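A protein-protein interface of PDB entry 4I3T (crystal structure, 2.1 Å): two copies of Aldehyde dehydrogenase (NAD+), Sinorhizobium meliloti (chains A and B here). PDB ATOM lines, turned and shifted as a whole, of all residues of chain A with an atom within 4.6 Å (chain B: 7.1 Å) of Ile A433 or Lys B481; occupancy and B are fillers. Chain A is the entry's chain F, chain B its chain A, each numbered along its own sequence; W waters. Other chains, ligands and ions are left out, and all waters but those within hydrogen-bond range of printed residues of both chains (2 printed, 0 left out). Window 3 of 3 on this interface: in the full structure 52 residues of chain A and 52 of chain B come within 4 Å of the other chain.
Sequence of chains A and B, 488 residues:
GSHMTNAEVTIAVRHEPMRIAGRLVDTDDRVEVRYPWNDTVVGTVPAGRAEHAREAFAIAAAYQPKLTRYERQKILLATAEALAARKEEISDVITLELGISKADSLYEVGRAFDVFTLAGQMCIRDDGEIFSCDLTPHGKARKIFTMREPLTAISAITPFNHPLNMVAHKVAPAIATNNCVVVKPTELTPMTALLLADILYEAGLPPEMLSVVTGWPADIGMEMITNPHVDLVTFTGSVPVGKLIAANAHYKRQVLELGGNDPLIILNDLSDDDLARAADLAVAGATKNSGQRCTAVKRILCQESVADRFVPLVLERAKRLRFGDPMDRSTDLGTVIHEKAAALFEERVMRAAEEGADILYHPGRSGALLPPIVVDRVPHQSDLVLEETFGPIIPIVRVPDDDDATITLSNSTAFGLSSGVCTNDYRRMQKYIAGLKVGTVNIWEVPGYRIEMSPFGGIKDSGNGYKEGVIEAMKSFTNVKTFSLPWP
The backbone NH (N) of Thr B482 is in hydrogen-bond range of the backbone carbonyl oxygen (O) of Gly A439, 2.7 Å away.
O of Thr B482 is in hydrogen-bond range of N of Val A441, at 2.8 Å.
O of Val A441 is in hydrogen-bond range of N of Ser B484, at 2.9 Å.
O of Leu A436 sits at hydrogen-bond distance from NZ of Lys B481 (2.6 Å).
O of Ser B484 lies within hydrogen-bond range of N of Ile A443 (2.8 Å).
The side-chain amino group (NZ) of Lys B481 sits at hydrogen-bond distance from the backbone carbonyl oxygen (O) of Ala A434 (3.3 Å).
The side-chain amino group (NZ) of Lys B481 lies within hydrogen-bond range of the backbone carbonyl oxygen (O) of Ile A433, at 3.0 Å.
The backbone NH (N) of Asn B479 is in hydrogen-bond range of the backbone carbonyl oxygen (O) of Glu B149 (2.8 Å).
OE2 of Glu B149 is in salt-bridge range of NZ of Lys B481 (2.8 Å).
The backbone NH of Lys B481 sits at hydrogen-bond distance from the backbone carbonyl oxygen of Met B147 (2.7 Å).
The backbone carbonyl oxygen (O) of Phe B483 sits at hydrogen-bond distance from the backbone NH (N) of Phe B145 (2.7 Å).
CG of Phe B483 touches CG2 of Ile A433, at 3.5 Å.
O of Ala A434 touches OE2 of Glu B149, 3.7 Å away.
O of Val A438 touches CE of Lys B481, 3.3 Å away.
O of Gly A439 touches O of Val B480, at 3.9 Å.
CA of Lys B481 touches O of Gly A439 (3.3 Å).
Phe B483 touches Val A441 (CA to O, 3.0 Å).
CG1 of Ile A443 touches CD2 of Leu B485, 3.5 Å away.
Gln A430 touches none of the printed residues of chain B.
Of chain B, only Lys B481 and Phe B483 come within 4 Å of Ile A433.
Of the printed residues of chain B, Gly A439 touches Val B480 (3.9 Å), Lys B481 (3.3 Å) and Thr B482 (2.7 Å).
Printed residues of chain B within 4 Å of Ile A443: Ser B484 and Leu B485.
Arg B148 touches none of the printed residues of chain A.
Lys B481 touches just these residues of chain A: Ile A433, Ala A434, Leu A436, Val A438 and Gly A439.
Printed residues of chain A within 4 Å of Ser B484: Val A441 (2.9 Å) and Ile A443 (2.8 Å).
Of the printed residues of chain A, Leu B485 touches Ile A443 (3.5 Å).
The nearest printed residue of chain A that does not touch Lys B481 is Gly A435 (4.5 Å).
The nearest printed residue of chain A that does not touch Thr B482 is Ile A433 (5.7 Å).
Of the 12 printed residues of chain A, 7 touch a printed residue of chain B.
Of the 13 printed residues of chain B, 7 touch a printed residue of chain A.
Printed residues of chain B that touch a printed residue of chain A: Glu B149, Val B480, Lys B481, Thr B482, Phe B483, Ser B484 and Leu B485.
Along chain B the printed residues that touch a printed residue of chain A span positions 149 to 485.
Among the printed residues, no Asp or Glu carboxylate lies within 4 Å of a Lys or Arg side-chain nitrogen of the other chain.
No position is printed for both chains.
Of the 14 pairs that touch across the chains among the printed residues, none has its exchanged pair printed and touching as well.
Water W1 bridges the side-chain carboxylate of Glu B149 (2.7 Å) and the backbone carbonyl oxygen of Ala A434 (3.2 Å).
Water W2 bridges the backbone carbonyl oxygen of Ala A434 (3.2 Å) and the side-chain amino group of Lys B481 (3.5 Å).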
ATOM      1  N   MET A 429     -20.371  -0.993  -6.273  1.00  0.00           N
ATOM      2  CA  MET A 429     -20.946   0.342  -6.396  1.00  0.00           C
ATOM      3  C   MET A 429     -22.434   0.216  -6.692  1.00  0.00           C
ATOM      4  O   MET A 429     -23.268   0.772  -5.985  1.00  0.00           O
ATOM      5  CB  MET A 429     -20.305   1.062  -7.569  1.00  0.00           C
ATOM      6  CG  MET A 429     -19.477   2.246  -7.228  1.00  0.00           C
ATOM      7  SD  MET A 429     -18.568   2.731  -8.706  1.00  0.00           S
ATOM      8  CE  MET A 429     -16.904   2.834  -8.029  1.00  0.00           C
ATOM      9  N   GLN A 430     -22.753  -0.510  -7.765  1.00  0.00           N
ATOM     10  CA  GLN A 430     -24.123  -0.601  -8.251  1.00  0.00           C
ATOM     11  C   GLN A 430     -24.993  -1.320  -7.229  1.00  0.00           C
ATOM     12  O   GLN A 430     -26.163  -1.000  -7.040  1.00  0.00           O
ATOM     13  CB  GLN A 430     -24.167  -1.323  -9.603  1.00  0.00           C
ATOM     14  CG  GLN A 430     -25.527  -1.269 -10.317  1.00  0.00           C
ATOM     15  CD  GLN A 430     -26.522  -2.300  -9.790  1.00  0.00           C
ATOM     16  OE1 GLN A 430     -26.144  -3.278  -9.134  1.00  0.00           O
ATOM     17  NE2 GLN A 430     -27.798  -2.084 -10.072  1.00  0.00           N
ATOM     18  N   LYS A 431     -24.407  -2.278  -6.529  1.00  0.00           N
ATOM     19  CA  LYS A 431     -25.154  -2.976  -5.499  1.00  0.00           C
ATOM     20  C   LYS A 431     -25.548  -2.032  -4.372  1.00  0.00           C
ATOM     21  O   LYS A 431     -26.677  -2.074  -3.871  1.00  0.00           O
ATOM     22  CB  LYS A 431     -24.333  -4.142  -4.955  1.00  0.00           C
ATOM     23  CG  LYS A 431     -25.017  -4.963  -3.868  1.00  0.00           C
ATOM     24  CD  LYS A 431     -24.057  -6.077  -3.419  1.00  0.00           C
ATOM     25  CE  LYS A 431     -24.634  -6.946  -2.317  1.00  0.00           C
ATOM     26  NZ  LYS A 431     -25.680  -7.895  -2.811  1.00  0.00           N
ATOM     27  N   TYR A 432     -24.627  -1.177  -3.948  1.00  0.00           N
ATOM     28  CA  TYR A 432     -24.977  -0.214  -2.906  1.00  0.00           C
ATOM     29  C   TYR A 432     -25.949   0.860  -3.432  1.00  0.00           C
ATOM     30  O   TYR A 432     -26.873   1.266  -2.731  1.00  0.00           O
ATOM     31  CB  TYR A 432     -23.726   0.439  -2.315  1.00  0.00           C
ATOM     32  CG  TYR A 432     -23.025  -0.437  -1.304  1.00  0.00           C
ATOM     33  CD1 TYR A 432     -22.202  -1.476  -1.709  1.00  0.00           C
ATOM     34  CD2 TYR A 432     -23.198  -0.225   0.060  1.00  0.00           C
ATOM     35  CE1 TYR A 432     -21.565  -2.287  -0.774  1.00  0.00           C
ATOM     36  CE2 TYR A 432     -22.579  -1.029   0.995  1.00  0.00           C
ATOM     37  CZ  TYR A 432     -21.757  -2.056   0.575  1.00  0.00           C
ATOM     38  OH  TYR A 432     -21.129  -2.864   1.509  1.00  0.00           O
ATOM     39  N   ILE A 433     -25.738   1.333  -4.657  1.00  0.00           N
ATOM     40  CA  ILE A 433     -26.654   2.334  -5.200  1.00  0.00           C
ATOM     41  C   ILE A 433     -28.082   1.774  -5.168  1.00  0.00           C
ATOM     42  O   ILE A 433     -29.010   2.428  -4.700  1.00  0.00           O
ATOM     43  CB  ILE A 433     -26.254   2.776  -6.620  1.00  0.00           C
ATOM     44  CG1 ILE A 433     -24.950   3.580  -6.555  1.00  0.00           C
ATOM     45  CG2 ILE A 433     -27.383   3.598  -7.251  1.00  0.00           C
ATOM     46  CD1 ILE A 433     -24.295   3.792  -7.894  1.00  0.00           C
ATOM     47  N   ALA A 434     -28.240   0.532  -5.611  1.00  0.00           N
ATOM     48  CA  ALA A 434     -29.563  -0.071  -5.652  1.00  0.00           C
ATOM     49  C   ALA A 434     -30.084  -0.420  -4.261  1.00  0.00           C
ATOM     50  O   ALA A 434     -31.273  -0.300  -3.994  1.00  0.00           O
ATOM     51  CB  ALA A 434     -29.577  -1.324  -6.558  1.00  0.00           C
ATOM     52  N   GLY A 435     -29.185  -0.830  -3.373  1.00  0.00           N
ATOM     53  CA  GLY A 435     -29.594  -1.413  -2.108  1.00  0.00           C
ATOM     54  C   GLY A 435     -29.769  -0.493  -0.915  1.00  0.00           C
ATOM     55  O   GLY A 435     -30.486  -0.835   0.029  1.00  0.00           O
ATOM     56  N   LEU A 436     -29.117   0.665  -0.920  1.00  0.00           N
ATOM     57  CA  LEU A 436     -29.261   1.587   0.207  1.00  0.00           C
ATOM     58  C   LEU A 436     -30.617   2.270   0.144  1.00  0.00           C
ATOM     59  O   LEU A 436     -31.059   2.712  -0.925  1.00  0.00           O
ATOM     60  CB  LEU A 436     -28.142   2.626   0.196  1.00  0.00           C
ATOM     61  CG  LEU A 436     -26.744   2.049   0.426  1.00  0.00           C
ATOM     62  CD1 LEU A 436     -25.678   3.135   0.242  1.00  0.00           C
ATOM     63  CD2 LEU A 436     -26.669   1.433   1.818  1.00  0.00           C
ATOM     64  N   VAL A 438     -32.215   5.223   0.676  1.00  0.00           N
ATOM     65  CA  VAL A 438     -31.904   6.621   0.908  1.00  0.00           C
ATOM     66  C   VAL A 438     -32.336   7.402  -0.339  1.00  0.00           C
ATOM     67  O   VAL A 438     -32.684   6.796  -1.354  1.00  0.00           O
ATOM     68  CB  VAL A 438     -30.372   6.805   1.112  1.00  0.00           C
ATOM     69  CG1 VAL A 438     -29.915   6.088   2.401  1.00  0.00           C
ATOM     70  CG2 VAL A 438     -29.618   6.245  -0.062  1.00  0.00           C
ATOM     71  N   GLY A 439     -32.319   8.734  -0.255  1.00  0.00           N
ATOM     72  CA  GLY A 439     -32.637   9.574  -1.394  1.00  0.00           C
ATOM     73  C   GLY A 439     -31.474   9.763  -2.343  1.00  0.00           C
ATOM     74  O   GLY A 439     -31.683  10.007  -3.531  1.00  0.00           O
ATOM     75  N   VAL A 441     -27.199   8.430  -3.217  1.00  0.00           N
ATOM     76  CA  VAL A 441     -26.001   7.637  -2.981  1.00  0.00           C
ATOM     77  C   VAL A 441     -24.846   8.232  -3.762  1.00  0.00           C
ATOM     78  O   VAL A 441     -24.826   8.132  -5.001  1.00  0.00           O
ATOM     79  CB  VAL A 441     -26.167   6.170  -3.459  1.00  0.00           C
ATOM     80  CG1 VAL A 441     -24.874   5.366  -3.184  1.00  0.00           C
ATOM     81  CG2 VAL A 441     -27.344   5.519  -2.793  1.00  0.00           C
ATOM     82  N   ILE A 443     -20.994   8.094  -4.861  1.00  0.00           N
ATOM     83  CA  ILE A 443     -19.793   7.264  -4.937  1.00  0.00           C
ATOM     84  C   ILE A 443     -18.557   8.141  -4.820  1.00  0.00           C
ATOM     85  O   ILE A 443     -18.376   9.078  -5.600  1.00  0.00           O
ATOM     86  CB  ILE A 443     -19.767   6.460  -6.217  1.00  0.00           C
ATOM     87  CG1 ILE A 443     -21.037   5.615  -6.318  1.00  0.00           C
ATOM     88  CG2 ILE A 443     -18.514   5.593  -6.316  1.00  0.00           C
ATOM     89  CD1 ILE A 443     -21.277   4.689  -5.132  1.00  0.00           C
ATOM     90  N   ILE B 144     -24.488  13.251 -11.599  1.00  0.00           N
ATOM     91  CA  ILE B 144     -25.589  12.774 -10.775  1.00  0.00           C
ATOM     92  C   ILE B 144     -26.627  12.163 -11.707  1.00  0.00           C
ATOM     93  O   ILE B 144     -26.896  12.710 -12.771  1.00  0.00           O
ATOM     94  CB  ILE B 144     -26.216  13.921  -9.973  1.00  0.00           C
ATOM     95  CG1 ILE B 144     -25.193  14.478  -8.982  1.00  0.00           C
ATOM     96  CG2 ILE B 144     -27.494  13.451  -9.254  1.00  0.00           C
ATOM     97  CD1 ILE B 144     -25.638  15.796  -8.363  1.00  0.00           C
ATOM     98  N   PHE B 145     -27.170  11.017 -11.318  1.00  0.00           N
ATOM     99  CA  PHE B 145     -28.169  10.309 -12.098  1.00  0.00           C
ATOM    100  C   PHE B 145     -29.380  10.101 -11.197  1.00  0.00           C
ATOM    101  O   PHE B 145     -29.284  10.072  -9.968  1.00  0.00           O
ATOM    102  CB  PHE B 145     -27.666   8.941 -12.549  1.00  0.00           C
ATOM    103  CG  PHE B 145     -26.372   8.981 -13.279  1.00  0.00           C
ATOM    104  CD1 PHE B 145     -25.169   9.062 -12.579  1.00  0.00           C
ATOM    105  CD2 PHE B 145     -26.345   8.945 -14.673  1.00  0.00           C
ATOM    106  CE1 PHE B 145     -23.959   9.113 -13.248  1.00  0.00           C
ATOM    107  CE2 PHE B 145     -25.132   8.992 -15.363  1.00  0.00           C
ATOM    108  CZ  PHE B 145     -23.931   9.050 -14.645  1.00  0.00           C
ATOM    109  N   THR B 146     -30.514   9.929 -11.841  1.00  0.00           N
ATOM    110  CA  THR B 146     -31.796   9.942 -11.186  1.00  0.00           C
ATOM    111  C   THR B 146     -32.550   8.658 -11.565  1.00  0.00           C
ATOM    112  O   THR B 146     -32.416   8.159 -12.674  1.00  0.00           O
ATOM    113  CB  THR B 146     -32.495  11.206 -11.686  1.00  0.00           C
ATOM    114  OG1 THR B 146     -32.497  12.209 -10.654  1.00  0.00           O
ATOM    115  CG2 THR B 146     -33.814  10.923 -12.162  1.00  0.00           C
ATOM    116  N   MET B 147     -33.333   8.123 -10.638  1.00  0.00           N
ATOM    117  CA  MET B 147     -33.932   6.815 -10.813  1.00  0.00           C
ATOM    118  C   MET B 147     -35.162   6.718  -9.901  1.00  0.00           C
ATOM    119  O   MET B 147     -35.245   7.422  -8.888  1.00  0.00           O
ATOM    120  CB  MET B 147     -32.845   5.778 -10.510  1.00  0.00           C
ATOM    121  CG  MET B 147     -33.230   4.499  -9.856  1.00  0.00           C
ATOM    122  SD  MET B 147     -31.669   3.681  -9.450  1.00  0.00           S
ATOM    123  CE  MET B 147     -32.155   2.748  -8.002  1.00  0.00           C
ATOM    124  N   ARG B 148     -36.124   5.870 -10.248  1.00  0.00           N
ATOM    125  CA  ARG B 148     -37.320   5.743  -9.415  1.00  0.00           C
ATOM    126  C   ARG B 148     -37.469   4.378  -8.763  1.00  0.00           C
ATOM    127  O   ARG B 148     -37.162   3.361  -9.374  1.00  0.00           O
ATOM    128  CB  ARG B 148     -38.581   6.074 -10.216  1.00  0.00           C
ATOM    129  CG  ARG B 148     -38.660   7.528 -10.624  1.00  0.00           C
ATOM    130  CD  ARG B 148     -39.883   7.789 -11.464  1.00  0.00           C
ATOM    131  NE  ARG B 148     -39.944   9.192 -11.839  1.00  0.00           N
ATOM    132  CZ  ARG B 148     -40.418  10.142 -11.049  1.00  0.00           C
ATOM    133  NH1 ARG B 148     -40.872   9.838  -9.827  1.00  0.00           N
ATOM    134  NH2 ARG B 148     -40.416  11.390 -11.471  1.00  0.00           N
ATOM    135  N   GLU B 149     -37.974   4.374  -7.535  1.00  0.00           N
ATOM    136  CA  GLU B 149     -38.248   3.136  -6.802  1.00  0.00           C
ATOM    137  C   GLU B 149     -39.654   3.159  -6.225  1.00  0.00           C
ATOM    138  O   GLU B 149     -40.171   4.228  -5.911  1.00  0.00           O
ATOM    139  CB  GLU B 149     -37.229   2.945  -5.674  1.00  0.00           C
ATOM    140  CG  GLU B 149     -35.820   2.710  -6.185  1.00  0.00           C
ATOM    141  CD  GLU B 149     -34.779   2.639  -5.066  1.00  0.00           C
ATOM    142  OE1 GLU B 149     -35.073   3.070  -3.934  1.00  0.00           O
ATOM    143  OE2 GLU B 149     -33.661   2.149  -5.336  1.00  0.00           O
ATOM    144  N   ASN B 479     -40.562   6.901  -5.327  1.00  0.00           N
ATOM    145  CA  ASN B 479     -39.576   7.785  -4.734  1.00  0.00           C
ATOM    146  C   ASN B 479     -38.446   7.936  -5.734  1.00  0.00           C
ATOM    147  O   ASN B 479     -38.034   6.959  -6.383  1.00  0.00           O
ATOM    148  CB  ASN B 479     -39.013   7.178  -3.440  1.00  0.00           C
ATOM    149  CG  ASN B 479     -40.012   7.203  -2.301  1.00  0.00           C
ATOM    150  OD1 ASN B 479     -40.714   8.197  -2.101  1.00  0.00           O
ATOM    151  ND2 ASN B 479     -40.081   6.102  -1.551  1.00  0.00           N
ATOM    152  N   VAL B 480     -37.940   9.151  -5.862  1.00  0.00           N
ATOM    153  CA  VAL B 480     -36.793   9.389  -6.707  1.00  0.00           C
ATOM    154  C   VAL B 480     -35.538   9.175  -5.878  1.00  0.00           C
ATOM    155  O   VAL B 480     -35.395   9.733  -4.797  1.00  0.00           O
ATOM    156  CB  VAL B 480     -36.801  10.833  -7.279  1.00  0.00           C
ATOM    157  CG1 VAL B 480     -35.464  11.153  -7.958  1.00  0.00           C
ATOM    158  CG2 VAL B 480     -37.983  11.014  -8.277  1.00  0.00           C
ATOM    159  N   LYS B 481     -34.636   8.352  -6.380  1.00  0.00           N
ATOM    160  CA  LYS B 481     -33.323   8.192  -5.772  1.00  0.00           C
ATOM    161  C   LYS B 481     -32.288   8.788  -6.723  1.00  0.00           C
ATOM    162  O   LYS B 481     -32.331   8.550  -7.941  1.00  0.00           O
ATOM    163  CB  LYS B 481     -33.018   6.703  -5.513  1.00  0.00           C
ATOM    164  CG  LYS B 481     -31.605   6.429  -5.002  1.00  0.00           C
ATOM    165  CD  LYS B 481     -31.328   4.931  -4.861  1.00  0.00           C
ATOM    166  CE  LYS B 481     -31.815   4.398  -3.496  1.00  0.00           C
ATOM    167  NZ  LYS B 481     -31.709   2.899  -3.431  1.00  0.00           N
ATOM    168  N   THR B 482     -31.364   9.583  -6.189  1.00  0.00           N
ATOM    169  CA  THR B 482     -30.241  10.025  -7.010  1.00  0.00           C
ATOM    170  C   THR B 482     -28.975   9.268  -6.620  1.00  0.00           C
ATOM    171  O   THR B 482     -28.827   8.824  -5.473  1.00  0.00           O
ATOM    172  CB  THR B 482     -29.965  11.531  -6.842  1.00  0.00           C
ATOM    173  OG1 THR B 482     -29.384  11.768  -5.554  1.00  0.00           O
ATOM    174  CG2 THR B 482     -31.268  12.326  -6.974  1.00  0.00           C
ATOM    175  N   PHE B 483     -28.054   9.133  -7.574  1.00  0.00           N
ATOM    176  CA  PHE B 483     -26.714   8.638  -7.262  1.00  0.00           C
ATOM    177  C   PHE B 483     -25.692   9.380  -8.094  1.00  0.00           C
ATOM    178  O   PHE B 483     -25.993   9.852  -9.212  1.00  0.00           O
ATOM    179  CB  PHE B 483     -26.590   7.116  -7.459  1.00  0.00           C
ATOM    180  CG  PHE B 483     -26.883   6.642  -8.870  1.00  0.00           C
ATOM    181  CD1 PHE B 483     -28.181   6.362  -9.278  1.00  0.00           C
ATOM    182  CD2 PHE B 483     -25.851   6.461  -9.770  1.00  0.00           C
ATOM    183  CE1 PHE B 483     -28.431   5.907 -10.555  1.00  0.00           C
ATOM    184  CE2 PHE B 483     -26.094   5.995 -11.050  1.00  0.00           C
ATOM    185  CZ  PHE B 483     -27.391   5.723 -11.440  1.00  0.00           C
ATOM    186  N   SER B 484     -24.485   9.515  -7.559  1.00  0.00           N
ATOM    187  CA  SER B 484     -23.451  10.265  -8.261  1.00  0.00           C
ATOM    188  C   SER B 484     -22.189   9.439  -8.408  1.00  0.00           C
ATOM    189  O   SER B 484     -21.830   8.643  -7.526  1.00  0.00           O
ATOM    190  CB  SER B 484     -23.148  11.626  -7.599  1.00  0.00           C
ATOM    191  OG  SER B 484     -22.499  11.476  -6.343  1.00  0.00           O
ATOM    192  N   LEU B 485     -21.536   9.609  -9.554  1.00  0.00           N
ATOM    193  CA  LEU B 485     -20.337   8.841  -9.876  1.00  0.00           C
ATOM    194  C   LEU B 485     -19.200   9.777 -10.228  1.00  0.00           C
ATOM    195  O   LEU B 485     -19.412  10.788 -10.901  1.00  0.00           O
ATOM    196  CB  LEU B 485     -20.580   7.929 -11.081  1.00  0.00           C
ATOM    197  CG  LEU B 485     -21.678   6.870 -10.926  1.00  0.00           C
ATOM    198  CD1 LEU B 485     -21.828   6.122 -12.255  1.00  0.00           C
ATOM    199  CD2 LEU B 485     -21.333   5.915  -9.796  1.00  0.00           C
HETATM  200  O   HOH W   1     -33.154  -0.138  -6.590  1.00  0.00           O
HETATM  201  O   HOH W   2     -33.668   0.414  -2.019  1.00  0.00           O
